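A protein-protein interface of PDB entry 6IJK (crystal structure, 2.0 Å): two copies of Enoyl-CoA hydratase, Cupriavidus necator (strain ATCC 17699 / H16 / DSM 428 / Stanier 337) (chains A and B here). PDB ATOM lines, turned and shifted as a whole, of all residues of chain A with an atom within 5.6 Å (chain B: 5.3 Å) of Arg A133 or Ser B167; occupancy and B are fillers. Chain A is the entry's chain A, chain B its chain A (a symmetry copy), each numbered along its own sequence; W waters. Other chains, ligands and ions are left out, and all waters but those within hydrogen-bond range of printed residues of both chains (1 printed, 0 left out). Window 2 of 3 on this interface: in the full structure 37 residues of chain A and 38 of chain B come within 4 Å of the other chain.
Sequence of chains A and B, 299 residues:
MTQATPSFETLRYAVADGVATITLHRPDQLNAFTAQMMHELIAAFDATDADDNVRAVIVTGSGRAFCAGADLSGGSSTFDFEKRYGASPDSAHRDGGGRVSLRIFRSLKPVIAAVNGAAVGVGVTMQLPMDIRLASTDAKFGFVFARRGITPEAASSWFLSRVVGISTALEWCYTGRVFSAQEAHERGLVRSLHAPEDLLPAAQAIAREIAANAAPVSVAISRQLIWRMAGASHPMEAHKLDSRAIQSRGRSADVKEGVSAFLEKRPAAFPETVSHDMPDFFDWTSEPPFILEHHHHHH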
ATOM      1  N   ILE A 112     -23.013  23.108 -31.226  1.00  0.00           N
ATOM      2  CA  ILE A 112     -24.069  22.916 -30.189  1.00  0.00           C
ATOM      3  C   ILE A 112     -25.310  22.419 -30.924  1.00  0.00           C
ATOM      4  O   ILE A 112     -25.765  23.138 -31.893  1.00  0.00           O
ATOM      5  CB  ILE A 112     -24.313  24.263 -29.482  1.00  0.00           C
ATOM      6  CG1 ILE A 112     -23.078  24.717 -28.703  1.00  0.00           C
ATOM      7  CG2 ILE A 112     -25.556  24.186 -28.609  1.00  0.00           C
ATOM      8  CD1 ILE A 112     -22.988  26.222 -28.491  1.00  0.00           C
ATOM      9  N   ALA A 113     -25.899  21.302 -30.510  1.00  0.00           N
ATOM     10  CA  ALA A 113     -27.233  20.896 -30.998  1.00  0.00           C
ATOM     11  C   ALA A 113     -28.313  21.574 -30.129  1.00  0.00           C
ATOM     12  O   ALA A 113     -28.237  21.517 -28.869  1.00  0.00           O
ATOM     13  CB  ALA A 113     -27.378  19.417 -31.032  1.00  0.00           C
ATOM     14  N   VAL A 115     -31.944  20.800 -29.821  1.00  0.00           N
ATOM     15  CA  VAL A 115     -32.892  19.718 -30.163  1.00  0.00           C
ATOM     16  C   VAL A 115     -34.303  20.193 -29.804  1.00  0.00           C
ATOM     17  O   VAL A 115     -34.654  20.168 -28.630  1.00  0.00           O
ATOM     18  CB  VAL A 115     -32.527  18.418 -29.452  1.00  0.00           C
ATOM     19  CG1 VAL A 115     -33.489  17.322 -29.878  1.00  0.00           C
ATOM     20  CG2 VAL A 115     -31.065  18.034 -29.730  1.00  0.00           C
ATOM     21  N   GLN A 127     -26.248  13.829 -33.369  1.00  0.00           N
ATOM     22  CA  GLN A 127     -25.913  14.817 -32.301  1.00  0.00           C
ATOM     23  C   GLN A 127     -24.704  14.375 -31.455  1.00  0.00           C
ATOM     24  O   GLN A 127     -24.122  15.202 -30.706  1.00  0.00           O
ATOM     25  CB  GLN A 127     -27.067  14.973 -31.306  1.00  0.00           C
ATOM     26  CG  GLN A 127     -28.420  15.198 -31.927  1.00  0.00           C
ATOM     27  CD  GLN A 127     -29.537  15.166 -30.914  1.00  0.00           C
ATOM     28  OE1 GLN A 127     -30.699  14.985 -31.269  1.00  0.00           O
ATOM     29  NE2 GLN A 127     -29.213  15.421 -29.662  1.00  0.00           N
ATOM     30  N   LEU A 128     -24.329  13.112 -31.497  1.00  0.00           N
ATOM     31  CA  LEU A 128     -23.385  12.579 -30.475  1.00  0.00           C
ATOM     32  C   LEU A 128     -21.995  13.162 -30.713  1.00  0.00           C
ATOM     33  O   LEU A 128     -21.283  13.433 -29.737  1.00  0.00           O
ATOM     34  CB  LEU A 128     -23.442  11.048 -30.492  1.00  0.00           C
ATOM     35  CG  LEU A 128     -24.839  10.442 -30.397  1.00  0.00           C
ATOM     36  CD1 LEU A 128     -24.752   8.940 -30.600  1.00  0.00           C
ATOM     37  CD2 LEU A 128     -25.527  10.738 -29.052  1.00  0.00           C
ATOM     38  N   PRO A 129     -21.565  13.413 -31.995  1.00  0.00           N
ATOM     39  CA  PRO A 129     -20.287  14.077 -32.272  1.00  0.00           C
ATOM     40  C   PRO A 129     -20.268  15.577 -32.032  1.00  0.00           C
ATOM     41  O   PRO A 129     -19.256  16.148 -31.909  1.00  0.00           O
ATOM     42  CB  PRO A 129     -20.040  13.824 -33.769  1.00  0.00           C
ATOM     43  CG  PRO A 129     -20.906  12.616 -34.070  1.00  0.00           C
ATOM     44  CD  PRO A 129     -22.134  12.802 -33.197  1.00  0.00           C
ATOM     45  N   MET A 130     -21.434  16.170 -31.902  1.00  0.00           N
ATOM     46  CA  MET A 130     -21.517  17.578 -31.529  1.00  0.00           C
ATOM     47  C   MET A 130     -21.023  17.672 -30.091  1.00  0.00           C
ATOM     48  O   MET A 130     -20.775  16.635 -29.434  1.00  0.00           O
ATOM     49  CB  MET A 130     -22.934  18.104 -31.748  1.00  0.00           C
ATOM     50  CG  MET A 130     -23.393  17.834 -33.185  1.00  0.00           C
ATOM     51  SD  MET A 130     -25.052  18.429 -33.527  1.00  0.00           S
ATOM     52  CE  MET A 130     -25.327  17.749 -35.180  1.00  0.00           C
ATOM     53  N   ASP A 131     -20.741  18.891 -29.681  1.00  0.00           N
ATOM     54  CA  ASP A 131     -19.926  19.165 -28.483  1.00  0.00           C
ATOM     55  C   ASP A 131     -20.852  19.320 -27.290  1.00  0.00           C
ATOM     56  O   ASP A 131     -20.442  18.929 -26.176  1.00  0.00           O
ATOM     57  CB  ASP A 131     -19.046  20.383 -28.731  1.00  0.00           C
ATOM     58  CG  ASP A 131     -18.132  20.201 -29.928  1.00  0.00           C
ATOM     59  OD1 ASP A 131     -17.812  19.038 -30.200  1.00  0.00           O
ATOM     60  OD2 ASP A 131     -17.758  21.219 -30.563  1.00  0.00           O
ATOM     61  N   ILE A 132     -22.012  19.924 -27.516  1.00  0.00           N
ATOM     62  CA  ILE A 132     -23.015  20.260 -26.455  1.00  0.00           C
ATOM     63  C   ILE A 132     -24.408  20.011 -27.035  1.00  0.00           C
ATOM     64  O   ILE A 132     -24.680  20.477 -28.150  1.00  0.00           O
ATOM     65  CB  ILE A 132     -22.835  21.708 -25.976  1.00  0.00           C
ATOM     66  CG1 ILE A 132     -21.430  21.927 -25.397  1.00  0.00           C
ATOM     67  CG2 ILE A 132     -23.923  22.106 -24.991  1.00  0.00           C
ATOM     68  CD1 ILE A 132     -21.122  23.371 -25.040  1.00  0.00           C
ATOM     69  N   ARG A 133     -25.244  19.269 -26.314  1.00  0.00           N
ATOM     70  CA  ARG A 133     -26.649  19.015 -26.689  1.00  0.00           C
ATOM     71  C   ARG A 133     -27.530  19.775 -25.697  1.00  0.00           C
ATOM     72  O   ARG A 133     -27.425  19.478 -24.501  1.00  0.00           O
ATOM     73  CB  ARG A 133     -26.885  17.503 -26.727  1.00  0.00           C
ATOM     74  CG  ARG A 133     -26.202  16.810 -27.907  1.00  0.00           C
ATOM     75  CD  ARG A 133     -26.015  15.303 -27.665  1.00  0.00           C
ATOM     76  NE  ARG A 133     -25.031  15.242 -26.628  1.00  0.00           N
ATOM     77  CZ  ARG A 133     -23.740  15.375 -26.840  1.00  0.00           C
ATOM     78  NH1 ARG A 133     -23.301  15.416 -28.083  1.00  0.00           N
ATOM     79  NH2 ARG A 133     -22.898  15.340 -25.827  1.00  0.00           N
ATOM     80  N   LEU A 134     -28.307  20.738 -26.176  1.00  0.00           N
ATOM     81  CA  LEU A 134     -29.418  21.397 -25.440  1.00  0.00           C
ATOM     82  C   LEU A 134     -30.723  20.864 -25.993  1.00  0.00           C
ATOM     83  O   LEU A 134     -30.783  20.713 -27.232  1.00  0.00           O
ATOM     84  CB  LEU A 134     -29.384  22.896 -25.697  1.00  0.00           C
ATOM     85  CG  LEU A 134     -28.545  23.713 -24.736  1.00  0.00           C
ATOM     86  CD1 LEU A 134     -27.165  23.118 -24.566  1.00  0.00           C
ATOM     87  CD2 LEU A 134     -28.497  25.147 -25.237  1.00  0.00           C
ATOM     88  N   ALA A 135     -31.748  20.666 -25.151  1.00  0.00           N
ATOM     89  CA  ALA A 135     -33.025  20.094 -25.618  1.00  0.00           C
ATOM     90  C   ALA A 135     -34.156  21.003 -25.148  1.00  0.00           C
ATOM     91  O   ALA A 135     -34.081  21.503 -23.985  1.00  0.00           O
ATOM     92  CB  ALA A 135     -33.225  18.695 -25.097  1.00  0.00           C
ATOM     93  N   VAL A 163     -20.827   9.589 -24.451  1.00  0.00           N
ATOM     94  CA  VAL A 163     -21.771  10.632 -23.976  1.00  0.00           C
ATOM     95  C   VAL A 163     -22.489  10.129 -22.732  1.00  0.00           C
ATOM     96  O   VAL A 163     -22.577  10.865 -21.772  1.00  0.00           O
ATOM     97  CB  VAL A 163     -22.786  10.967 -25.074  1.00  0.00           C
ATOM     98  CG1 VAL A 163     -23.737  12.053 -24.612  1.00  0.00           C
ATOM     99  CG2 VAL A 163     -22.092  11.351 -26.359  1.00  0.00           C
ATOM    100  N   GLY A 188     -27.599  11.906 -19.078  1.00  0.00           N
ATOM    101  CA  GLY A 188     -26.464  12.719 -19.534  1.00  0.00           C
ATOM    102  C   GLY A 188     -26.380  12.876 -21.047  1.00  0.00           C
ATOM    103  O   GLY A 188     -25.362  13.433 -21.470  1.00  0.00           O
ATOM    104  N   LEU A 189     -27.403  12.501 -21.848  1.00  0.00           N
ATOM    105  CA  LEU A 189     -27.393  12.819 -23.317  1.00  0.00           C
ATOM    106  C   LEU A 189     -27.413  14.347 -23.557  1.00  0.00           C
ATOM    107  O   LEU A 189     -26.744  14.846 -24.487  1.00  0.00           O
ATOM    108  CB  LEU A 189     -28.569  12.102 -24.013  1.00  0.00           C
ATOM    109  CG  LEU A 189     -28.708  12.348 -25.521  1.00  0.00           C
ATOM    110  CD1 LEU A 189     -27.450  11.946 -26.294  1.00  0.00           C
ATOM    111  CD2 LEU A 189     -29.909  11.625 -26.090  1.00  0.00           C
ATOM    112  N   VAL A 190     -28.145  15.106 -22.742  1.00  0.00           N
ATOM    113  CA  VAL A 190     -28.273  16.573 -22.955  1.00  0.00           C
ATOM    114  C   VAL A 190     -27.791  17.331 -21.717  1.00  0.00           C
ATOM    115  O   VAL A 190     -27.991  16.868 -20.554  1.00  0.00           O
ATOM    116  CB  VAL A 190     -29.704  16.964 -23.371  1.00  0.00           C
ATOM    117  CG1 VAL A 190     -30.133  16.224 -24.641  1.00  0.00           C
ATOM    118  CG2 VAL A 190     -30.717  16.765 -22.258  1.00  0.00           C
ATOM    119  N   ARG A 191     -27.131  18.450 -21.979  1.00  0.00           N
ATOM    120  CA  ARG A 191     -26.520  19.314 -20.958  1.00  0.00           C
ATOM    121  C   ARG A 191     -27.642  19.919 -20.099  1.00  0.00           C
ATOM    122  O   ARG A 191     -27.500  19.949 -18.883  1.00  0.00           O
ATOM    123  CB  ARG A 191     -25.707  20.383 -21.684  1.00  0.00           C
ATOM    124  CG  ARG A 191     -25.161  21.455 -20.765  1.00  0.00           C
ATOM    125  CD  ARG A 191     -24.905  22.728 -21.518  1.00  0.00           C
ATOM    126  NE  ARG A 191     -24.311  23.785 -20.714  1.00  0.00           N
ATOM    127  CZ  ARG A 191     -24.977  24.804 -20.179  1.00  0.00           C
ATOM    128  NH1 ARG A 191     -26.292  24.899 -20.283  1.00  0.00           N
ATOM    129  NH2 ARG A 191     -24.315  25.736 -19.525  1.00  0.00           N
ATOM    130  N   SER A 192     -28.673  20.452 -20.733  1.00  0.00           N
ATOM    131  CA  SER A 192     -29.744  21.250 -20.081  1.00  0.00           C
ATOM    132  C   SER A 192     -31.052  21.218 -20.894  1.00  0.00           C
ATOM    133  O   SER A 192     -31.049  20.874 -22.134  1.00  0.00           O
ATOM    134  CB  SER A 192     -29.291  22.676 -19.806  1.00  0.00           C
ATOM    135  OG  SER A 192     -28.681  23.264 -20.946  1.00  0.00           O
ATOM    136  N   GLY B 165     -16.179  13.648 -18.636  1.00  0.00           N
ATOM    137  CA  GLY B 165     -16.800  13.333 -19.926  1.00  0.00           C
ATOM    138  C   GLY B 165     -16.621  14.468 -20.905  1.00  0.00           C
ATOM    139  O   GLY B 165     -16.420  15.686 -20.473  1.00  0.00           O
ATOM    140  N   ILE B 166     -16.690  14.101 -22.180  1.00  0.00           N
ATOM    141  CA  ILE B 166     -16.211  14.961 -23.290  1.00  0.00           C
ATOM    142  C   ILE B 166     -17.035  16.253 -23.357  1.00  0.00           C
ATOM    143  O   ILE B 166     -16.451  17.330 -23.563  1.00  0.00           O
ATOM    144  CB  ILE B 166     -16.223  14.172 -24.608  1.00  0.00           C
ATOM    145  CG1 ILE B 166     -15.137  13.101 -24.608  1.00  0.00           C
ATOM    146  CG2 ILE B 166     -16.043  15.131 -25.768  1.00  0.00           C
ATOM    147  CD1 ILE B 166     -15.115  12.265 -25.848  1.00  0.00           C
ATOM    148  N   SER B 167     -18.359  16.177 -23.277  1.00  0.00           N
ATOM    149  CA  SER B 167     -19.203  17.367 -23.526  1.00  0.00           C
ATOM    150  C   SER B 167     -18.905  18.465 -22.497  1.00  0.00           C
ATOM    151  O   SER B 167     -18.752  19.691 -22.847  1.00  0.00           O
ATOM    152  CB  SER B 167     -20.679  17.028 -23.507  1.00  0.00           C
ATOM    153  OG  SER B 167     -21.415  18.228 -23.738  1.00  0.00           O
ATOM    154  N   THR B 168     -18.907  18.091 -21.228  1.00  0.00           N
ATOM    155  CA  THR B 168     -18.510  19.044 -20.170  1.00  0.00           C
ATOM    156  C   THR B 168     -17.068  19.574 -20.383  1.00  0.00           C
ATOM    157  O   THR B 168     -16.829  20.775 -20.074  1.00  0.00           O
ATOM    158  CB  THR B 168     -18.674  18.437 -18.772  1.00  0.00           C
ATOM    159  OG1 THR B 168     -20.051  18.150 -18.534  1.00  0.00           O
ATOM    160  CG2 THR B 168     -18.186  19.396 -17.715  1.00  0.00           C
ATOM    161  N   ALA B 169     -16.124  18.742 -20.796  1.00  0.00           N
ATOM    162  CA  ALA B 169     -14.720  19.153 -20.991  1.00  0.00           C
ATOM    163  C   ALA B 169     -14.676  20.239 -22.068  1.00  0.00           C
ATOM    164  O   ALA B 169     -13.993  21.276 -21.891  1.00  0.00           O
ATOM    165  CB  ALA B 169     -13.887  17.955 -21.363  1.00  0.00           C
ATOM    166  N   LEU B 170     -15.457  20.044 -23.118  1.00  0.00           N
ATOM    167  CA  LEU B 170     -15.481  20.947 -24.282  1.00  0.00           C
ATOM    168  C   LEU B 170     -16.074  22.281 -23.834  1.00  0.00           C
ATOM    169  O   LEU B 170     -15.501  23.303 -24.172  1.00  0.00           O
ATOM    170  CB  LEU B 170     -16.288  20.268 -25.392  1.00  0.00           C
ATOM    171  CG  LEU B 170     -15.537  19.150 -26.105  1.00  0.00           C
ATOM    172  CD1 LEU B 170     -16.481  18.358 -26.970  1.00  0.00           C
ATOM    173  CD2 LEU B 170     -14.344  19.699 -26.881  1.00  0.00           C
ATOM    174  N   GLU B 171     -17.130  22.260 -23.040  1.00  0.00           N
ATOM    175  CA  GLU B 171     -17.865  23.483 -22.654  1.00  0.00           C
ATOM    176  C   GLU B 171     -16.980  24.347 -21.741  1.00  0.00           C
ATOM    177  O   GLU B 171     -16.916  25.562 -21.928  1.00  0.00           O
ATOM    178  CB  GLU B 171     -19.184  23.144 -21.978  1.00  0.00           C
ATOM    179  CG  GLU B 171     -19.991  24.381 -21.646  1.00  0.00           C
ATOM    180  CD  GLU B 171     -21.227  24.120 -20.807  1.00  0.00           C
ATOM    181  OE1 GLU B 171     -21.712  22.986 -20.825  1.00  0.00           O
ATOM    182  OE2 GLU B 171     -21.730  25.077 -20.198  1.00  0.00           O
ATOM    183  N   TRP B 172     -16.354  23.730 -20.755  1.00  0.00           N
ATOM    184  CA  TRP B 172     -15.453  24.433 -19.818  1.00  0.00           C
ATOM    185  C   TRP B 172     -14.249  25.033 -20.567  1.00  0.00           C
ATOM    186  O   TRP B 172     -13.860  26.158 -20.229  1.00  0.00           O
ATOM    187  CB  TRP B 172     -15.021  23.448 -18.747  1.00  0.00           C
ATOM    188  CG  TRP B 172     -16.056  23.156 -17.719  1.00  0.00           C
ATOM    189  CD1 TRP B 172     -17.190  23.863 -17.441  1.00  0.00           C
ATOM    190  CD2 TRP B 172     -15.960  22.138 -16.717  1.00  0.00           C
ATOM    191  NE1 TRP B 172     -17.804  23.344 -16.333  1.00  0.00           N
ATOM    192  CE2 TRP B 172     -17.068  22.297 -15.857  1.00  0.00           C
ATOM    193  CE3 TRP B 172     -15.064  21.100 -16.447  1.00  0.00           C
ATOM    194  CZ2 TRP B 172     -17.309  21.423 -14.799  1.00  0.00           C
ATOM    195  CZ3 TRP B 172     -15.289  20.266 -15.376  1.00  0.00           C
ATOM    196  CH2 TRP B 172     -16.420  20.407 -14.584  1.00  0.00           C
HETATM  197  O   HOH W   1     -24.389  18.196 -23.840  1.00  0.00           O
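The backbone carbonyl oxygen (O) of Met A130 lies within hydrogen-bond range of the guanidinium group (NH1) of Arg A133 (3.1 Å). The guanidinium group (NH1) of Arg A133 is in hydrogen-bond range of the backbone carbonyl oxygen (O) of Leu A128, 3.3 Å away. The backbone carbonyl oxygen (O) of Gln A127 is in hydrogen-bond range of the guanidinium group (NH1) of Arg A133 (2.8 Å). The backbone NH of Arg A191 sits at hydrogen-bond distance from the backbone carbonyl oxygen of Arg A133. NH1 of Arg A191 sits at hydrogen-bond distance from OG of Ser A192 (3.0 Å). The backbone carbonyl oxygen (O) of Leu A189 lies within hydrogen-bond range of the guanidinium group (NE) of Arg A133 (2.8 Å).
Asp A131 touches Leu B170. OG of Ser B167 touches CA of Ile A132, at 3.8 Å. Ile A132 touches Glu B171 (CD1 to CB, 3.6 Å). Arg A133 touches Ser B167.
Water W1 lies within hydrogen-bond range of the backbone NH of Arg A133, the side-chain hydroxyl of Ser B167 and the backbone NH of Arg A191.
No position is printed for both chains.
Of the 8 printed residues of chain B, 3 touch a printed residue of chain A. Among the printed residues, 6 pairs touch across the chains. Among the printed residues, Asp or Glu carboxylates within 4 Å of a Lys or Arg side-chain nitrogen of the other chain: Arg A191 with Glu B171.
OG of Ser B167 sits at hydrogen-bond distance from O of Asp A131. OE1 of Glu B171 lies within salt-bridge range of NE of Arg A191 (2.7 Å).
Met A130 touches none of the printed residues of chain B. Printed residues of chain B within 4 Å of Ile A132: Ser B167 (3.8 Å) and Glu B171 (3.6 Å). Arg A133 touches just one residue of chain B: Ser B167. Val A190 touches none of the printed residues of chain B. Ser B167 touches just these residues of chain A: Asp A131, Ile A132 and Arg A133. Of the printed residues of chain A, Glu B171 touches Ile A132 (3.6 Å) and Arg A191 (2.7 Å).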
